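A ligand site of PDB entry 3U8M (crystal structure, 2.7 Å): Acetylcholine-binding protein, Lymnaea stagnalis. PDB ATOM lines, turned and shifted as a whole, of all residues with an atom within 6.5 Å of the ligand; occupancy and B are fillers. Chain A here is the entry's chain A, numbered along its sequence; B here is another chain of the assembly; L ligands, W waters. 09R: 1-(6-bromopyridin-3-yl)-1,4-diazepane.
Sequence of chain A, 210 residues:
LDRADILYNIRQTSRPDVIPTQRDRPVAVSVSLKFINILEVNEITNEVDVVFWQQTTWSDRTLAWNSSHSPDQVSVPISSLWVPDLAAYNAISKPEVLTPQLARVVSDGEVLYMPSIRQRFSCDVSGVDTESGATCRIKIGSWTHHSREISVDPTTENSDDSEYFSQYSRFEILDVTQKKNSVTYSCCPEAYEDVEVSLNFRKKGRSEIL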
ATOM      1  N   TYR A  89       8.267  -7.161 -14.566  1.00  0.00           N
ATOM      2  CA  TYR A  89       7.868  -5.774 -14.322  1.00  0.00           C
ATOM      3  C   TYR A  89       8.381  -4.775 -15.365  1.00  0.00           C
ATOM      4  O   TYR A  89       7.662  -3.867 -15.790  1.00  0.00           O
ATOM      5  CB  TYR A  89       8.318  -5.338 -12.919  1.00  0.00           C
ATOM      6  CG  TYR A  89       7.431  -5.882 -11.811  1.00  0.00           C
ATOM      7  CD1 TYR A  89       7.393  -7.243 -11.540  1.00  0.00           C
ATOM      8  CD2 TYR A  89       6.624  -5.042 -11.059  1.00  0.00           C
ATOM      9  CE1 TYR A  89       6.590  -7.741 -10.535  1.00  0.00           C
ATOM     10  CE2 TYR A  89       5.822  -5.526 -10.054  1.00  0.00           C
ATOM     11  CZ  TYR A  89       5.800  -6.882  -9.801  1.00  0.00           C
ATOM     12  OH  TYR A  89       5.003  -7.396  -8.811  1.00  0.00           O
ATOM     13  N   SER A 142       4.957 -12.584  -9.101  1.00  0.00           N
ATOM     14  CA  SER A 142       3.533 -12.759  -9.292  1.00  0.00           C
ATOM     15  C   SER A 142       2.908 -11.390  -9.484  1.00  0.00           C
ATOM     16  O   SER A 142       3.285 -10.432  -8.796  1.00  0.00           O
ATOM     17  CB  SER A 142       2.894 -13.469  -8.098  1.00  0.00           C
ATOM     18  OG  SER A 142       1.482 -13.444  -8.187  1.00  0.00           O
ATOM     19  N   TRP A 143       1.946 -11.297 -10.388  1.00  0.00           N
ATOM     20  CA  TRP A 143       1.315 -10.021 -10.648  1.00  0.00           C
ATOM     21  C   TRP A 143       0.235  -9.678  -9.616  1.00  0.00           C
ATOM     22  O   TRP A 143       0.155  -8.535  -9.146  1.00  0.00           O
ATOM     23  CB  TRP A 143       0.742  -9.963 -12.068  1.00  0.00           C
ATOM     24  CG  TRP A 143       0.513  -8.570 -12.545  1.00  0.00           C
ATOM     25  CD1 TRP A 143      -0.691  -7.983 -12.802  1.00  0.00           C
ATOM     26  CD2 TRP A 143       1.503  -7.588 -12.795  1.00  0.00           C
ATOM     27  NE1 TRP A 143      -0.507  -6.677 -13.200  1.00  0.00           N
ATOM     28  CE2 TRP A 143       0.844  -6.417 -13.202  1.00  0.00           C
ATOM     29  CE3 TRP A 143       2.902  -7.582 -12.710  1.00  0.00           C
ATOM     30  CZ2 TRP A 143       1.523  -5.253 -13.530  1.00  0.00           C
ATOM     31  CZ3 TRP A 143       3.572  -6.417 -13.023  1.00  0.00           C
ATOM     32  CH2 TRP A 143       2.882  -5.263 -13.438  1.00  0.00           C
ATOM     33  N   THR A 144      -0.572 -10.667  -9.242  1.00  0.00           N
ATOM     34  CA  THR A 144      -1.734 -10.401  -8.396  1.00  0.00           C
ATOM     35  C   THR A 144      -1.705 -11.124  -7.052  1.00  0.00           C
ATOM     36  O   THR A 144      -2.483 -10.778  -6.150  1.00  0.00           O
ATOM     37  CB  THR A 144      -3.048 -10.753  -9.134  1.00  0.00           C
ATOM     38  OG1 THR A 144      -3.044 -12.134  -9.481  1.00  0.00           O
ATOM     39  CG2 THR A 144      -3.198  -9.928 -10.395  1.00  0.00           C
ATOM     40  N   HIS A 145      -0.830 -12.126  -6.904  1.00  0.00           N
ATOM     41  CA  HIS A 145      -0.741 -12.908  -5.668  1.00  0.00           C
ATOM     42  C   HIS A 145       0.357 -12.426  -4.722  1.00  0.00           C
ATOM     43  O   HIS A 145       1.542 -12.469  -5.071  1.00  0.00           O
ATOM     44  CB  HIS A 145      -0.517 -14.388  -5.957  1.00  0.00           C
ATOM     45  CG  HIS A 145      -1.663 -15.053  -6.635  1.00  0.00           C
ATOM     46  ND1 HIS A 145      -2.835 -15.358  -5.978  1.00  0.00           N
ATOM     47  CD2 HIS A 145      -1.813 -15.497  -7.902  1.00  0.00           C
ATOM     48  CE1 HIS A 145      -3.665 -15.959  -6.823  1.00  0.00           C
ATOM     49  NE2 HIS A 145      -3.061 -16.058  -7.996  1.00  0.00           N
ATOM     50  N   VAL A 183       8.149  -6.774  -1.764  1.00  0.00           N
ATOM     51  CA  VAL A 183       7.851  -5.362  -1.976  1.00  0.00           C
ATOM     52  C   VAL A 183       6.395  -5.035  -1.663  1.00  0.00           C
ATOM     53  O   VAL A 183       5.492  -5.785  -2.006  1.00  0.00           O
ATOM     54  CB  VAL A 183       8.142  -4.952  -3.452  1.00  0.00           C
ATOM     55  CG1 VAL A 183       7.816  -3.494  -3.670  1.00  0.00           C
ATOM     56  CG2 VAL A 183       9.573  -5.227  -3.816  1.00  0.00           C
ATOM     57  N   TYR A 185       3.374  -2.387  -2.492  1.00  0.00           N
ATOM     58  CA  TYR A 185       3.056  -1.388  -3.510  1.00  0.00           C
ATOM     59  C   TYR A 185       1.915  -0.466  -3.051  1.00  0.00           C
ATOM     60  O   TYR A 185       1.057  -0.867  -2.270  1.00  0.00           O
ATOM     61  CB  TYR A 185       2.725  -2.066  -4.859  1.00  0.00           C
ATOM     62  CG  TYR A 185       3.859  -2.924  -5.367  1.00  0.00           C
ATOM     63  CD1 TYR A 185       4.080  -4.195  -4.859  1.00  0.00           C
ATOM     64  CD2 TYR A 185       4.716  -2.475  -6.344  1.00  0.00           C
ATOM     65  CE1 TYR A 185       5.118  -4.975  -5.307  1.00  0.00           C
ATOM     66  CE2 TYR A 185       5.758  -3.249  -6.805  1.00  0.00           C
ATOM     67  CZ  TYR A 185       5.959  -4.503  -6.276  1.00  0.00           C
ATOM     68  OH  TYR A 185       6.996  -5.298  -6.724  1.00  0.00           O
ATOM     69  N   CYS A 187      -0.835   0.566  -4.330  1.00  0.00           N
ATOM     70  CA  CYS A 187      -2.212   0.107  -4.525  1.00  0.00           C
ATOM     71  C   CYS A 187      -2.773  -0.749  -3.374  1.00  0.00           C
ATOM     72  O   CYS A 187      -3.986  -0.718  -3.113  1.00  0.00           O
ATOM     73  CB  CYS A 187      -2.292  -0.731  -5.800  1.00  0.00           C
ATOM     74  SG  CYS A 187      -1.777  -2.456  -5.540  1.00  0.00           S
ATOM     75  N   CYS A 188      -1.918  -1.522  -2.719  1.00  0.00           N
ATOM     76  CA  CYS A 188      -2.370  -2.645  -1.910  1.00  0.00           C
ATOM     77  C   CYS A 188      -1.587  -2.753  -0.613  1.00  0.00           C
ATOM     78  O   CYS A 188      -0.425  -2.367  -0.553  1.00  0.00           O
ATOM     79  CB  CYS A 188      -2.247  -3.954  -2.707  1.00  0.00           C
ATOM     80  SG  CYS A 188      -2.780  -3.819  -4.429  1.00  0.00           S
ATOM     81  N   GLU A 190      -0.812  -5.565   1.063  1.00  0.00           N
ATOM     82  CA  GLU A 190       0.028  -6.756   1.174  1.00  0.00           C
ATOM     83  C   GLU A 190       1.366  -6.601   0.476  1.00  0.00           C
ATOM     84  O   GLU A 190       1.560  -5.694  -0.333  1.00  0.00           O
ATOM     85  CB  GLU A 190      -0.717  -7.985   0.634  1.00  0.00           C
ATOM     86  CG  GLU A 190      -1.938  -8.367   1.442  1.00  0.00           C
ATOM     87  CD  GLU A 190      -1.600  -9.181   2.681  1.00  0.00           C
ATOM     88  OE1 GLU A 190      -0.395  -9.254   3.029  1.00  0.00           O
ATOM     89  OE2 GLU A 190      -2.522  -9.768   3.295  1.00  0.00           O
ATOM     90  N   TYR A 192       4.271  -8.174  -2.059  1.00  0.00           N
ATOM     91  CA  TYR A 192       4.366  -9.047  -3.220  1.00  0.00           C
ATOM     92  C   TYR A 192       5.815  -9.380  -3.496  1.00  0.00           C
ATOM     93  O   TYR A 192       6.680  -8.507  -3.483  1.00  0.00           O
ATOM     94  CB  TYR A 192       3.713  -8.407  -4.441  1.00  0.00           C
ATOM     95  CG  TYR A 192       2.228  -8.156  -4.284  1.00  0.00           C
ATOM     96  CD1 TYR A 192       1.769  -7.097  -3.508  1.00  0.00           C
ATOM     97  CD2 TYR A 192       1.283  -8.983  -4.910  1.00  0.00           C
ATOM     98  CE1 TYR A 192       0.399  -6.869  -3.351  1.00  0.00           C
ATOM     99  CE2 TYR A 192      -0.072  -8.749  -4.771  1.00  0.00           C
ATOM    100  CZ  TYR A 192      -0.521  -7.699  -3.989  1.00  0.00           C
ATOM    101  OH  TYR A 192      -1.869  -7.473  -3.854  1.00  0.00           O
ATOM    102  N   TRP B  53       0.296   1.010 -15.919  1.00  0.00           N
ATOM    103  CA  TRP B  53      -0.624   0.109 -15.244  1.00  0.00           C
ATOM    104  C   TRP B  53      -1.957   0.808 -15.291  1.00  0.00           C
ATOM    105  O   TRP B  53      -2.042   1.979 -14.873  1.00  0.00           O
ATOM    106  CB  TRP B  53      -0.234  -0.088 -13.789  1.00  0.00           C
ATOM    107  CG  TRP B  53       1.038  -0.842 -13.605  1.00  0.00           C
ATOM    108  CD1 TRP B  53       1.820  -1.382 -14.562  1.00  0.00           C
ATOM    109  CD2 TRP B  53       1.649  -1.156 -12.348  1.00  0.00           C
ATOM    110  NE1 TRP B  53       2.902  -2.007 -13.984  1.00  0.00           N
ATOM    111  CE2 TRP B  53       2.820  -1.881 -12.634  1.00  0.00           C
ATOM    112  CE3 TRP B  53       1.331  -0.879 -11.024  1.00  0.00           C
ATOM    113  CZ2 TRP B  53       3.660  -2.335 -11.636  1.00  0.00           C
ATOM    114  CZ3 TRP B  53       2.162  -1.325 -10.031  1.00  0.00           C
ATOM    115  CH2 TRP B  53       3.331  -2.042 -10.339  1.00  0.00           C
ATOM    116  N   SER B  75      -7.999 -14.440  -7.026  1.00  0.00           N
ATOM    117  CA  SER B  75      -7.664 -13.942  -8.353  1.00  0.00           C
ATOM    118  C   SER B  75      -8.504 -14.687  -9.377  1.00  0.00           C
ATOM    119  O   SER B  75      -8.582 -15.910  -9.379  1.00  0.00           O
ATOM    120  CB  SER B  75      -6.171 -14.096  -8.652  1.00  0.00           C
ATOM    121  OG  SER B  75      -5.403 -13.244  -7.809  1.00  0.00           O
ATOM    122  N   LEU B 102      -5.632 -11.241 -14.923  1.00  0.00           N
ATOM    123  CA  LEU B 102      -6.314 -11.646 -13.705  1.00  0.00           C
ATOM    124  C   LEU B 102      -6.848 -10.456 -12.943  1.00  0.00           C
ATOM    125  O   LEU B 102      -6.183  -9.449 -12.774  1.00  0.00           O
ATOM    126  CB  LEU B 102      -5.361 -12.429 -12.809  1.00  0.00           C
ATOM    127  CG  LEU B 102      -4.818 -13.718 -13.426  1.00  0.00           C
ATOM    128  CD1 LEU B 102      -3.956 -14.452 -12.451  1.00  0.00           C
ATOM    129  CD2 LEU B 102      -5.999 -14.589 -13.821  1.00  0.00           C
ATOM    130  N   ALA B 103      -8.086 -10.569 -12.478  1.00  0.00           N
ATOM    131  CA  ALA B 103      -8.636  -9.554 -11.584  1.00  0.00           C
ATOM    132  C   ALA B 103      -8.522 -10.059 -10.158  1.00  0.00           C
ATOM    133  O   ALA B 103      -8.265 -11.230  -9.916  1.00  0.00           O
ATOM    134  CB  ALA B 103     -10.081  -9.257 -11.919  1.00  0.00           C
ATOM    135  N   ARG B 104      -8.715  -9.154  -9.227  1.00  0.00           N
ATOM    136  CA  ARG B 104      -8.717  -9.537  -7.830  1.00  0.00           C
ATOM    137  C   ARG B 104     -10.111  -9.251  -7.261  1.00  0.00           C
ATOM    138  O   ARG B 104     -10.608  -8.133  -7.359  1.00  0.00           O
ATOM    139  CB  ARG B 104      -7.638  -8.762  -7.092  1.00  0.00           C
ATOM    140  CG  ARG B 104      -7.333  -9.278  -5.724  1.00  0.00           C
ATOM    141  CD  ARG B 104      -6.629 -10.624  -5.756  1.00  0.00           C
ATOM    142  NE  ARG B 104      -6.289 -11.002  -4.386  1.00  0.00           N
ATOM    143  CZ  ARG B 104      -5.597 -12.093  -4.068  1.00  0.00           C
ATOM    144  NH1 ARG B 104      -5.168 -12.929  -5.018  1.00  0.00           N
ATOM    145  NH2 ARG B 104      -5.336 -12.340  -2.787  1.00  0.00           N
ATOM    146  N   VAL B 105     -10.746 -10.275  -6.714  1.00  0.00           N
ATOM    147  CA  VAL B 105     -12.099 -10.116  -6.204  1.00  0.00           C
ATOM    148  C   VAL B 105     -12.172 -10.297  -4.698  1.00  0.00           C
ATOM    149  O   VAL B 105     -11.704 -11.306  -4.160  1.00  0.00           O
ATOM    150  CB  VAL B 105     -13.054 -11.084  -6.877  1.00  0.00           C
ATOM    151  CG1 VAL B 105     -14.471 -10.818  -6.431  1.00  0.00           C
ATOM    152  CG2 VAL B 105     -12.939 -10.938  -8.383  1.00  0.00           C
ATOM    153  N   LEU B 112     -10.575  -5.359  -8.289  1.00  0.00           N
ATOM    154  CA  LEU B 112      -9.417  -4.616  -8.784  1.00  0.00           C
ATOM    155  C   LEU B 112      -8.937  -5.341 -10.007  1.00  0.00           C
ATOM    156  O   LEU B 112      -8.820  -6.568 -10.012  1.00  0.00           O
ATOM    157  CB  LEU B 112      -8.258  -4.497  -7.741  1.00  0.00           C
ATOM    158  CG  LEU B 112      -6.983  -3.762  -8.237  1.00  0.00           C
ATOM    159  CD1 LEU B 112      -7.294  -2.321  -8.584  1.00  0.00           C
ATOM    160  CD2 LEU B 112      -5.752  -3.781  -7.301  1.00  0.00           C
ATOM    161  N   TYR B 113      -8.682  -4.580 -11.063  1.00  0.00           N
ATOM    162  CA  TYR B 113      -7.978  -5.083 -12.225  1.00  0.00           C
ATOM    163  C   TYR B 113      -6.931  -4.017 -12.564  1.00  0.00           C
ATOM    164  O   TYR B 113      -7.256  -2.836 -12.718  1.00  0.00           O
ATOM    165  CB  TYR B 113      -8.937  -5.336 -13.391  1.00  0.00           C
ATOM    166  CG  TYR B 113      -8.294  -5.896 -14.649  1.00  0.00           C
ATOM    167  CD1 TYR B 113      -7.398  -6.952 -14.591  1.00  0.00           C
ATOM    168  CD2 TYR B 113      -8.606  -5.364 -15.903  1.00  0.00           C
ATOM    169  CE1 TYR B 113      -6.799  -7.470 -15.738  1.00  0.00           C
ATOM    170  CE2 TYR B 113      -8.028  -5.879 -17.062  1.00  0.00           C
ATOM    171  CZ  TYR B 113      -7.121  -6.929 -16.964  1.00  0.00           C
ATOM    172  OH  TYR B 113      -6.549  -7.429 -18.109  1.00  0.00           O
ATOM    173  N   MET B 114      -5.674  -4.436 -12.655  1.00  0.00           N
ATOM    174  CA  MET B 114      -4.565  -3.520 -12.954  1.00  0.00           C
ATOM    175  C   MET B 114      -3.520  -4.150 -13.862  1.00  0.00           C
ATOM    176  O   MET B 114      -2.418  -4.473 -13.411  1.00  0.00           O
ATOM    177  CB  MET B 114      -3.919  -3.047 -11.663  1.00  0.00           C
ATOM    178  CG  MET B 114      -3.055  -1.848 -11.811  1.00  0.00           C
ATOM    179  SD  MET B 114      -2.712  -1.041 -10.240  1.00  0.00           S
ATOM    180  CE  MET B 114      -1.826  -2.343  -9.371  1.00  0.00           C
ATOM    181  N   PRO B 115      -3.856  -4.321 -15.150  1.00  0.00           N
ATOM    182  CA  PRO B 115      -2.897  -4.883 -16.092  1.00  0.00           C
ATOM    183  C   PRO B 115      -1.863  -3.816 -16.492  1.00  0.00           C
ATOM    184  O   PRO B 115      -2.142  -2.610 -16.456  1.00  0.00           O
ATOM    185  CB  PRO B 115      -3.767  -5.226 -17.293  1.00  0.00           C
ATOM    186  CG  PRO B 115      -4.798  -4.152 -17.276  1.00  0.00           C
ATOM    187  CD  PRO B 115      -5.101  -3.890 -15.816  1.00  0.00           C
ATOM    188  N   TYR B 164       6.386   4.465  -9.783  1.00  0.00           N
ATOM    189  CA  TYR B 164       6.761   3.218 -10.451  1.00  0.00           C
ATOM    190  C   TYR B 164       7.428   3.481 -11.791  1.00  0.00           C
ATOM    191  O   TYR B 164       7.533   2.581 -12.625  1.00  0.00           O
ATOM    192  CB  TYR B 164       5.538   2.304 -10.674  1.00  0.00           C
ATOM    193  CG  TYR B 164       4.715   2.025  -9.439  1.00  0.00           C
ATOM    194  CD1 TYR B 164       5.291   1.521  -8.286  1.00  0.00           C
ATOM    195  CD2 TYR B 164       3.344   2.259  -9.437  1.00  0.00           C
ATOM    196  CE1 TYR B 164       4.515   1.263  -7.160  1.00  0.00           C
ATOM    197  CE2 TYR B 164       2.559   2.001  -8.329  1.00  0.00           C
ATOM    198  CZ  TYR B 164       3.150   1.503  -7.194  1.00  0.00           C
ATOM    199  OH  TYR B 164       2.374   1.266  -6.089  1.00  0.00           O
HETATM  200  C1  09R L   1      -2.237  -5.841 -10.025  1.00  0.00           C
HETATM  201  C2  09R L   1      -1.609  -5.609  -8.771  1.00  0.00           C
HETATM  202  C3  09R L   1      -2.393  -5.972  -7.614  1.00  0.00           C
HETATM  203  C4  09R L   1      -3.703  -6.482  -7.787  1.00  0.00           C
HETATM  204  C5  09R L   1      -4.205  -6.654  -9.108  1.00  0.00           C
HETATM  205  N1  09R L   1      -3.470  -6.340 -10.189  1.00  0.00           N
HETATM  206 BR1  09R L   1      -5.793  -7.216  -9.485  1.00  0.00          BR
HETATM  207  N2  09R L   1      -0.339  -5.081  -8.788  1.00  0.00           N
HETATM  208  C6  09R L   1       0.496  -5.202  -9.983  1.00  0.00           C
HETATM  209  C7  09R L   1       1.982  -5.268  -9.610  1.00  0.00           C
HETATM  210  N3  09R L   1       2.292  -6.520  -8.922  1.00  0.00           N
HETATM  211  C8  09R L   1       2.238  -6.517  -7.426  1.00  0.00           C
HETATM  212  C9  09R L   1       1.202  -5.620  -6.708  1.00  0.00           C
HETATM  213  C10 09R L   1       0.349  -4.635  -7.552  1.00  0.00           C
HETATM  214  O   HOH W   1      -4.447  -7.042 -12.806  1.00  0.00           O
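A nitrogen (N3) of the ligand sits at hydrogen-bond distance from the backbone carbonyl oxygen (O) of Trp 143 (2.9 Å). A nitrogen (N3) of the ligand lies within hydrogen-bond range of the side-chain hydroxyl (OH) of Tyr 89.
The backbone carbonyl oxygen (O) of Ser 142 lies within hydrogen-bond range of the side-chain hydroxyl (OH) of Tyr 89. The backbone NH of Tyr 192 lies within hydrogen-bond range of the backbone carbonyl oxygen of Val 183 (2.7 Å). SG of Cys 187 is disulfide-bonded to SG of Cys 188, at 2.0 Å. The side-chain hydroxyl (OG) of Ser 75 of chain B sits at hydrogen-bond distance from the guanidinium group (NH1) of Arg 104 of chain B (2.8 Å). The backbone carbonyl oxygen (O) of Met 114 of chain B sits at hydrogen-bond distance from the indole nitrogen (NE1) of Trp 143. The side-chain hydroxyl of Thr 144 sits at hydrogen-bond distance from the side-chain hydroxyl of Ser 75 of chain B (3.1 Å). The backbone carbonyl oxygen (O) of Leu 112 of chain B is in hydrogen-bond range of the backbone NH (N) of Arg 104 of chain B (2.7 Å).
Residues that only touch the ligand: Thr 144, Tyr 185, Cys 187, Cys 188, Tyr 192, Trp 53 of chain B, Leu 102 of chain B, Ala 103 of chain B, Arg 104 of chain B, Leu 112 of chain B and Met 114 of chain B. Hydrophobic or aromatic side chains that line the ligand: Tyr 89, Trp 143, Tyr 185, Tyr 192, Trp 53 of chain B, Leu 112 of chain B and Met 114 of chain B. The nearest printed residue that does not touch the ligand is Ser 142 (4.04 Å).
Water W1 lies within hydrogen-bond range of a nitrogen (N1) of the ligand, the backbone NH (N) of Met 114 of chain B and the backbone carbonyl oxygen (O) of Leu 102 of chain B.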
